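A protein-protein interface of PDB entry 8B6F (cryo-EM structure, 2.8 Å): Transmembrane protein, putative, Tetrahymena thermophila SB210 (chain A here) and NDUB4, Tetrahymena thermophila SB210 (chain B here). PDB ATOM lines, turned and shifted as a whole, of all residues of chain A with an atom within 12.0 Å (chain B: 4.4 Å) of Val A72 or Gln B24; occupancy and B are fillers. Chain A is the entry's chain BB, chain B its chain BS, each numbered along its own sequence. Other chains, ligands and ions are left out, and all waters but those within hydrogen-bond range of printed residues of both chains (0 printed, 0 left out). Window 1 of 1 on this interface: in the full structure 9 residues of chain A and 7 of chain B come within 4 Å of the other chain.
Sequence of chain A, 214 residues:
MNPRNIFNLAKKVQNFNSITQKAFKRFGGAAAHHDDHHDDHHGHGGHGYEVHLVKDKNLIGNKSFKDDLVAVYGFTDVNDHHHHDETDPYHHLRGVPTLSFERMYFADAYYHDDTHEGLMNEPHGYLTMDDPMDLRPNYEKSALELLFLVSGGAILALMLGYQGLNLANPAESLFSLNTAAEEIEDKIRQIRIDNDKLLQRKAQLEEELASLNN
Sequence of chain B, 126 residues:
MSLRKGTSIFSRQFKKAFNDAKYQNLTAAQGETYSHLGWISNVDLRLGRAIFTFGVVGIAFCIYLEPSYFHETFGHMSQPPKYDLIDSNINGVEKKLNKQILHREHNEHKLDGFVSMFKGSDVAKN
The backbone carbonyl oxygen (O) of Ala A71 is in hydrogen-bond range of the side-chain amide nitrogen (NE2) of Gln B24, 2.9 Å away.
Val A70 touches Gln B24. Val A70 touches Leu B26 (O to CD2, 3.7 Å). O of Ala A71 touches O of Ala B21, 3.6 Å away. Val A72 touches Ala B17 (CG1 to CB, 3.98 Å). O of Val A72 touches CB of Ala B21 (3.0 Å). NE2 of Gln B24 touches O of Val A72, 3.8 Å away. Phe A75 touches Leu B26 (CD2 to O, 3.6 Å).
Of the printed residues of chain B, Val A70 touches Gln B24 and Leu B26. Of the printed residues of chain B, Ala A71 touches Ala B21 (3.6 Å) and Gln B24 (2.9 Å). Printed residues of chain B within 4 Å of Val A72: Ala B17, Ala B21 and Gln B24. Of the printed residues of chain B, Phe A75 touches Leu B26 (3.6 Å). Of the printed residues of chain A, Ala B17 touches Val A72 (3.98 Å). Ala B21 touches just these residues of chain A: Ala A71 (3.6 Å) and Val A72 (3.0 Å). Gln B24 touches three residues of chain A. No residue of chain A comes within 4 Å of Asn B25. Leu B26 touches just these residues of chain A: Val A70 (3.7 Å) and Phe A75 (3.6 Å). No residue of chain A comes within 4 Å of Thr B33. The nearest printed residue of chain B that does not touch Val A72 is Phe B18 (4.1 Å). The nearest printed residue of chain B that does not touch Phe A75 is Gln B24 (6.6 Å).
Of the 15 printed residues of chain A, 4 touch a printed residue of chain B. Printed residues of chain A that touch a printed residue of chain B: Val A70, Ala A71, Val A72 and Phe A75. Of the 11 printed residues of chain B, 4 touch a printed residue of chain A. Hydrophobic or aromatic side chains of chain B that line the printed part of chain A: Ala B17, Ala B21 and Leu B26. Among the printed residues, no Asp or Glu carboxylate lies within 4 Å of a Lys or Arg side-chain nitrogen of the other chain.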
ATOM      1  N   ASN A  62      -0.115 -11.475 -21.144  1.00  0.00           N
ATOM      2  CA  ASN A  62       0.621 -12.646 -21.600  1.00  0.00           C
ATOM      3  C   ASN A  62      -0.049 -13.917 -21.100  1.00  0.00           C
ATOM      4  O   ASN A  62      -0.393 -14.027 -19.920  1.00  0.00           O
ATOM      5  CB  ASN A  62       2.068 -12.582 -21.119  1.00  0.00           C
ATOM      6  CG  ASN A  62       2.795 -11.358 -21.631  1.00  0.00           C
ATOM      7  OD1 ASN A  62       3.163 -10.474 -20.860  1.00  0.00           O
ATOM      8  ND2 ASN A  62       3.005 -11.299 -22.941  1.00  0.00           N
ATOM      9  N   SER A  64       1.346 -16.974 -21.051  1.00  0.00           N
ATOM     10  CA  SER A  64       2.303 -17.753 -20.278  1.00  0.00           C
ATOM     11  C   SER A  64       3.688 -17.152 -20.457  1.00  0.00           C
ATOM     12  O   SER A  64       3.964 -16.463 -21.442  1.00  0.00           O
ATOM     13  CB  SER A  64       2.293 -19.227 -20.691  1.00  0.00           C
ATOM     14  OG  SER A  64       2.660 -19.376 -22.047  1.00  0.00           O
ATOM     15  N   PHE A  65       4.559 -17.425 -19.484  1.00  0.00           N
ATOM     16  CA  PHE A  65       5.923 -16.913 -19.535  1.00  0.00           C
ATOM     17  C   PHE A  65       6.800 -17.701 -20.500  1.00  0.00           C
ATOM     18  O   PHE A  65       7.685 -17.119 -21.135  1.00  0.00           O
ATOM     19  CB  PHE A  65       6.547 -16.934 -18.138  1.00  0.00           C
ATOM     20  CG  PHE A  65       7.890 -16.265 -18.065  1.00  0.00           C
ATOM     21  CD1 PHE A  65       9.046 -16.964 -18.371  1.00  0.00           C
ATOM     22  CD2 PHE A  65       7.995 -14.938 -17.689  1.00  0.00           C
ATOM     23  CE1 PHE A  65      10.281 -16.348 -18.304  1.00  0.00           C
ATOM     24  CE2 PHE A  65       9.227 -14.317 -17.621  1.00  0.00           C
ATOM     25  CZ  PHE A  65      10.370 -15.022 -17.928  1.00  0.00           C
ATOM     26  N   LYS A  66       6.584 -19.011 -20.619  1.00  0.00           N
ATOM     27  CA  LYS A  66       7.446 -19.830 -21.466  1.00  0.00           C
ATOM     28  C   LYS A  66       7.078 -19.684 -22.939  1.00  0.00           C
ATOM     29  O   LYS A  66       7.946 -19.418 -23.777  1.00  0.00           O
ATOM     30  CB  LYS A  66       7.362 -21.297 -21.039  1.00  0.00           C
ATOM     31  CG  LYS A  66       8.190 -21.650 -19.810  1.00  0.00           C
ATOM     32  CD  LYS A  66       7.688 -20.939 -18.562  1.00  0.00           C
ATOM     33  CE  LYS A  66       8.380 -21.464 -17.311  1.00  0.00           C
ATOM     34  NZ  LYS A  66       7.962 -20.719 -16.089  1.00  0.00           N
ATOM     35  N   ASP A  67       5.796 -19.854 -23.272  1.00  0.00           N
ATOM     36  CA  ASP A  67       5.388 -19.811 -24.673  1.00  0.00           C
ATOM     37  C   ASP A  67       5.692 -18.453 -25.294  1.00  0.00           C
ATOM     38  O   ASP A  67       6.177 -18.375 -26.428  1.00  0.00           O
ATOM     39  CB  ASP A  67       3.903 -20.143 -24.800  1.00  0.00           C
ATOM     40  CG  ASP A  67       3.538 -21.441 -24.110  1.00  0.00           C
ATOM     41  OD1 ASP A  67       4.416 -22.322 -24.000  1.00  0.00           O
ATOM     42  OD2 ASP A  67       2.377 -21.579 -23.672  1.00  0.00           O
ATOM     43  N   ASP A  68       5.407 -17.375 -24.572  1.00  0.00           N
ATOM     44  CA  ASP A  68       5.771 -16.035 -25.007  1.00  0.00           C
ATOM     45  C   ASP A  68       7.166 -15.715 -24.493  1.00  0.00           C
ATOM     46  O   ASP A  68       7.468 -15.944 -23.318  1.00  0.00           O
ATOM     47  CB  ASP A  68       4.771 -15.002 -24.487  1.00  0.00           C
ATOM     48  CG  ASP A  68       3.334 -15.422 -24.699  1.00  0.00           C
ATOM     49  OD1 ASP A  68       3.073 -16.188 -25.649  1.00  0.00           O
ATOM     50  OD2 ASP A  68       2.466 -14.991 -23.913  1.00  0.00           O
ATOM     51  N   LEU A  69       8.015 -15.183 -25.367  1.00  0.00           N
ATOM     52  CA  LEU A  69       9.384 -14.884 -24.977  1.00  0.00           C
ATOM     53  C   LEU A  69       9.415 -13.653 -24.082  1.00  0.00           C
ATOM     54  O   LEU A  69       9.942 -12.606 -24.467  1.00  0.00           O
ATOM     55  CB  LEU A  69      10.262 -14.680 -26.212  1.00  0.00           C
ATOM     56  CG  LEU A  69      10.397 -15.893 -27.134  1.00  0.00           C
ATOM     57  CD1 LEU A  69      11.273 -15.556 -28.323  1.00  0.00           C
ATOM     58  CD2 LEU A  69      10.956 -17.099 -26.392  1.00  0.00           C
ATOM     59  N   VAL A  70       8.848 -13.780 -22.882  1.00  0.00           N
ATOM     60  CA  VAL A  70       8.824 -12.661 -21.947  1.00  0.00           C
ATOM     61  C   VAL A  70      10.241 -12.248 -21.580  1.00  0.00           C
ATOM     62  O   VAL A  70      10.541 -11.056 -21.444  1.00  0.00           O
ATOM     63  CB  VAL A  70       7.999 -13.030 -20.700  1.00  0.00           C
ATOM     64  CG1 VAL A  70       8.114 -11.952 -19.634  1.00  0.00           C
ATOM     65  CG2 VAL A  70       6.544 -13.258 -21.075  1.00  0.00           C
ATOM     66  N   ALA A  71      11.135 -13.223 -21.414  1.00  0.00           N
ATOM     67  CA  ALA A  71      12.511 -12.907 -21.060  1.00  0.00           C
ATOM     68  C   ALA A  71      13.183 -12.025 -22.102  1.00  0.00           C
ATOM     69  O   ALA A  71      14.173 -11.357 -21.785  1.00  0.00           O
ATOM     70  CB  ALA A  71      13.312 -14.196 -20.875  1.00  0.00           C
ATOM     71  N   VAL A  72      12.674 -12.010 -23.329  1.00  0.00           N
ATOM     72  CA  VAL A  72      13.220 -11.176 -24.388  1.00  0.00           C
ATOM     73  C   VAL A  72      12.387  -9.919 -24.599  1.00  0.00           C
ATOM     74  O   VAL A  72      12.937  -8.825 -24.732  1.00  0.00           O
ATOM     75  CB  VAL A  72      13.336 -11.990 -25.696  1.00  0.00           C
ATOM     76  CG1 VAL A  72      13.969 -11.150 -26.796  1.00  0.00           C
ATOM     77  CG2 VAL A  72      14.140 -13.259 -25.465  1.00  0.00           C
ATOM     78  N   TYR A  73      11.061 -10.055 -24.630  1.00  0.00           N
ATOM     79  CA  TYR A  73      10.174  -8.937 -24.924  1.00  0.00           C
ATOM     80  C   TYR A  73       9.460  -8.389 -23.696  1.00  0.00           C
ATOM     81  O   TYR A  73       8.752  -7.383 -23.813  1.00  0.00           O
ATOM     82  CB  TYR A  73       9.130  -9.360 -25.962  1.00  0.00           C
ATOM     83  CG  TYR A  73       9.729  -9.907 -27.234  1.00  0.00           C
ATOM     84  CD1 TYR A  73      10.102  -9.062 -28.270  1.00  0.00           C
ATOM     85  CD2 TYR A  73       9.925 -11.269 -27.398  1.00  0.00           C
ATOM     86  CE1 TYR A  73      10.652  -9.559 -29.434  1.00  0.00           C
ATOM     87  CE2 TYR A  73      10.475 -11.777 -28.557  1.00  0.00           C
ATOM     88  CZ  TYR A  73      10.836 -10.917 -29.572  1.00  0.00           C
ATOM     89  OH  TYR A  73      11.383 -11.419 -30.729  1.00  0.00           O
ATOM     90  N   GLY A  74       9.616  -9.014 -22.536  1.00  0.00           N
ATOM     91  CA  GLY A  74       8.973  -8.517 -21.339  1.00  0.00           C
ATOM     92  C   GLY A  74       7.480  -8.809 -21.320  1.00  0.00           C
ATOM     93  O   GLY A  74       6.943  -9.569 -22.126  1.00  0.00           O
ATOM     94  N   PHE A  75       6.810  -8.176 -20.363  1.00  0.00           N
ATOM     95  CA  PHE A  75       5.379  -8.346 -20.157  1.00  0.00           C
ATOM     96  C   PHE A  75       4.609  -7.235 -20.857  1.00  0.00           C
ATOM     97  O   PHE A  75       5.016  -6.071 -20.832  1.00  0.00           O
ATOM     98  CB  PHE A  75       5.036  -8.335 -18.666  1.00  0.00           C
ATOM     99  CG  PHE A  75       5.534  -9.534 -17.916  1.00  0.00           C
ATOM    100  CD1 PHE A  75       4.826 -10.723 -17.936  1.00  0.00           C
ATOM    101  CD2 PHE A  75       6.695  -9.462 -17.166  1.00  0.00           C
ATOM    102  CE1 PHE A  75       5.277 -11.825 -17.237  1.00  0.00           C
ATOM    103  CE2 PHE A  75       7.152 -10.560 -16.464  1.00  0.00           C
ATOM    104  CZ  PHE A  75       6.441 -11.743 -16.498  1.00  0.00           C
ATOM    105  N   THR A  76       3.495  -7.602 -21.483  1.00  0.00           N
ATOM    106  CA  THR A  76       2.583  -6.631 -22.068  1.00  0.00           C
ATOM    107  C   THR A  76       1.581  -6.161 -21.021  1.00  0.00           C
ATOM    108  O   THR A  76       1.207  -6.908 -20.114  1.00  0.00           O
ATOM    109  CB  THR A  76       1.838  -7.225 -23.267  1.00  0.00           C
ATOM    110  OG1 THR A  76       1.122  -8.399 -22.860  1.00  0.00           O
ATOM    111  CG2 THR A  76       2.812  -7.583 -24.376  1.00  0.00           C
ATOM    112  N   ASP A  77       1.146  -4.912 -21.157  1.00  0.00           N
ATOM    113  CA  ASP A  77       0.240  -4.286 -20.207  1.00  0.00           C
ATOM    114  C   ASP A  77      -1.138  -4.110 -20.829  1.00  0.00           C
ATOM    115  O   ASP A  77      -1.260  -3.766 -22.008  1.00  0.00           O
ATOM    116  CB  ASP A  77       0.776  -2.926 -19.750  1.00  0.00           C
ATOM    117  CG  ASP A  77       2.038  -3.045 -18.919  1.00  0.00           C
ATOM    118  OD1 ASP A  77       2.477  -4.185 -18.662  1.00  0.00           O
ATOM    119  OD2 ASP A  77       2.591  -1.998 -18.520  1.00  0.00           O
ATOM    120  N   ALA B  17      16.977  -7.324 -30.022  1.00  0.00           N
ATOM    121  CA  ALA B  17      16.076  -7.479 -28.886  1.00  0.00           C
ATOM    122  C   ALA B  17      16.752  -8.245 -27.757  1.00  0.00           C
ATOM    123  O   ALA B  17      16.664  -7.857 -26.587  1.00  0.00           O
ATOM    124  CB  ALA B  17      14.796  -8.189 -29.327  1.00  0.00           C
ATOM    125  N   PHE B  18      17.432  -9.346 -28.090  1.00  0.00           N
ATOM    126  CA  PHE B  18      18.116 -10.126 -27.063  1.00  0.00           C
ATOM    127  C   PHE B  18      19.256  -9.338 -26.432  1.00  0.00           C
ATOM    128  O   PHE B  18      19.454  -9.395 -25.213  1.00  0.00           O
ATOM    129  CB  PHE B  18      18.639 -11.435 -27.648  1.00  0.00           C
ATOM    130  CG  PHE B  18      19.328 -12.306 -26.638  1.00  0.00           C
ATOM    131  CD1 PHE B  18      18.601 -13.179 -25.847  1.00  0.00           C
ATOM    132  CD2 PHE B  18      20.702 -12.244 -26.469  1.00  0.00           C
ATOM    133  CE1 PHE B  18      19.228 -13.977 -24.912  1.00  0.00           C
ATOM    134  CE2 PHE B  18      21.336 -13.038 -25.535  1.00  0.00           C
ATOM    135  CZ  PHE B  18      20.598 -13.907 -24.756  1.00  0.00           C
ATOM    136  N   ASP B  20      19.479  -6.135 -26.004  1.00  0.00           N
ATOM    137  CA  ASP B  20      18.912  -5.139 -25.108  1.00  0.00           C
ATOM    138  C   ASP B  20      18.198  -5.757 -23.914  1.00  0.00           C
ATOM    139  O   ASP B  20      18.064  -5.091 -22.882  1.00  0.00           O
ATOM    140  CB  ASP B  20      17.935  -4.244 -25.873  1.00  0.00           C
ATOM    141  CG  ASP B  20      18.593  -3.519 -27.028  1.00  0.00           C
ATOM    142  OD1 ASP B  20      19.815  -3.270 -26.958  1.00  0.00           O
ATOM    143  OD2 ASP B  20      17.890  -3.194 -28.007  1.00  0.00           O
ATOM    144  N   ALA B  21      17.740  -7.002 -24.023  1.00  0.00           N
ATOM    145  CA  ALA B  21      16.904  -7.613 -23.000  1.00  0.00           C
ATOM    146  C   ALA B  21      17.616  -8.662 -22.159  1.00  0.00           C
ATOM    147  O   ALA B  21      16.993  -9.234 -21.262  1.00  0.00           O
ATOM    148  CB  ALA B  21      15.669  -8.246 -23.649  1.00  0.00           C
ATOM    149  N   LYS B  22      18.895  -8.941 -22.418  1.00  0.00           N
ATOM    150  CA  LYS B  22      19.573  -9.971 -21.638  1.00  0.00           C
ATOM    151  C   LYS B  22      19.608  -9.615 -20.156  1.00  0.00           C
ATOM    152  O   LYS B  22      19.403 -10.482 -19.299  1.00  0.00           O
ATOM    153  CB  LYS B  22      20.987 -10.196 -22.167  1.00  0.00           C
ATOM    154  CG  LYS B  22      21.702 -11.347 -21.470  1.00  0.00           C
ATOM    155  CD  LYS B  22      23.057 -11.631 -22.085  1.00  0.00           C
ATOM    156  CE  LYS B  22      23.764 -12.751 -21.342  1.00  0.00           C
ATOM    157  NZ  LYS B  22      25.103 -13.041 -21.919  1.00  0.00           N
ATOM    158  N   TYR B  23      19.868  -8.347 -19.835  1.00  0.00           N
ATOM    159  CA  TYR B  23      20.000  -7.891 -18.456  1.00  0.00           C
ATOM    160  C   TYR B  23      18.921  -6.879 -18.087  1.00  0.00           C
ATOM    161  O   TYR B  23      19.162  -5.969 -17.294  1.00  0.00           O
ATOM    162  CB  TYR B  23      21.385  -7.292 -18.222  1.00  0.00           C
ATOM    163  CG  TYR B  23      22.516  -8.239 -18.535  1.00  0.00           C
ATOM    164  CD1 TYR B  23      22.822  -9.289 -17.682  1.00  0.00           C
ATOM    165  CD2 TYR B  23      23.289  -8.074 -19.676  1.00  0.00           C
ATOM    166  CE1 TYR B  23      23.857 -10.154 -17.959  1.00  0.00           C
ATOM    167  CE2 TYR B  23      24.328  -8.935 -19.962  1.00  0.00           C
ATOM    168  CZ  TYR B  23      24.607  -9.972 -19.098  1.00  0.00           C
ATOM    169  OH  TYR B  23      25.640 -10.835 -19.372  1.00  0.00           O
ATOM    170  N   GLN B  24      17.727  -7.027 -18.649  1.00  0.00           N
ATOM    171  CA  GLN B  24      16.648  -6.095 -18.376  1.00  0.00           C
ATOM    172  C   GLN B  24      16.025  -6.372 -17.010  1.00  0.00           C
ATOM    173  O   GLN B  24      16.234  -7.422 -16.397  1.00  0.00           O
ATOM    174  CB  GLN B  24      15.585  -6.177 -19.471  1.00  0.00           C
ATOM    175  CG  GLN B  24      14.868  -7.515 -19.536  1.00  0.00           C
ATOM    176  CD  GLN B  24      13.842  -7.565 -20.646  1.00  0.00           C
ATOM    177  OE1 GLN B  24      13.499  -6.542 -21.234  1.00  0.00           O
ATOM    178  NE2 GLN B  24      13.351  -8.759 -20.942  1.00  0.00           N
ATOM    179  N   ASN B  25      15.251  -5.402 -16.531  1.00  0.00           N
ATOM    180  CA  ASN B  25      14.493  -5.524 -15.289  1.00  0.00           C
ATOM    181  C   ASN B  25      13.074  -5.940 -15.662  1.00  0.00           C
ATOM    182  O   ASN B  25      12.263  -5.112 -16.084  1.00  0.00           O
ATOM    183  CB  ASN B  25      14.513  -4.208 -14.518  1.00  0.00           C
ATOM    184  CG  ASN B  25      13.799  -4.300 -13.188  1.00  0.00           C
ATOM    185  OD1 ASN B  25      13.797  -5.346 -12.544  1.00  0.00           O
ATOM    186  ND2 ASN B  25      13.184  -3.202 -12.770  1.00  0.00           N
ATOM    187  N   LEU B  26      12.774  -7.231 -15.508  1.00  0.00           N
ATOM    188  CA  LEU B  26      11.493  -7.758 -15.962  1.00  0.00           C
ATOM    189  C   LEU B  26      10.314  -7.212 -15.170  1.00  0.00           C
ATOM    190  O   LEU B  26       9.176  -7.305 -15.639  1.00  0.00           O
ATOM    191  CB  LEU B  26      11.502  -9.285 -15.890  1.00  0.00           C
ATOM    192  CG  LEU B  26      12.452  -9.986 -16.864  1.00  0.00           C
ATOM    193  CD1 LEU B  26      12.527 -11.472 -16.570  1.00  0.00           C
ATOM    194  CD2 LEU B  26      12.019  -9.758 -18.300  1.00  0.00           C
ATOM    195  N   THR B  33      12.557  -0.877 -19.080  1.00  0.00           N
ATOM    196  CA  THR B  33      13.144  -2.034 -18.406  1.00  0.00           C
ATOM    197  C   THR B  33      14.617  -2.168 -18.798  1.00  0.00           C
ATOM    198  O   THR B  33      15.041  -3.114 -19.460  1.00  0.00           O
ATOM    199  CB  THR B  33      12.353  -3.300 -18.736  1.00  0.00           C
ATOM    200  OG1 THR B  33      13.018  -4.442 -18.180  1.00  0.00           O
ATOM    201  CG2 THR B  33      12.206  -3.491 -20.245  1.00  0.00           C
ATOM    202  N   SER B  35      18.637  -1.550 -16.985  1.00  0.00           N
ATOM    203  CA  SER B  35      19.339  -1.446 -15.714  1.00  0.00           C
ATOM    204  C   SER B  35      20.614  -0.623 -15.778  1.00  0.00           C
ATOM    205  O   SER B  35      21.016  -0.057 -14.760  1.00  0.00           O
ATOM    206  CB  SER B  35      19.693  -2.847 -15.199  1.00  0.00           C
ATOM    207  OG  SER B  35      18.539  -3.667 -15.153  1.00  0.00           O
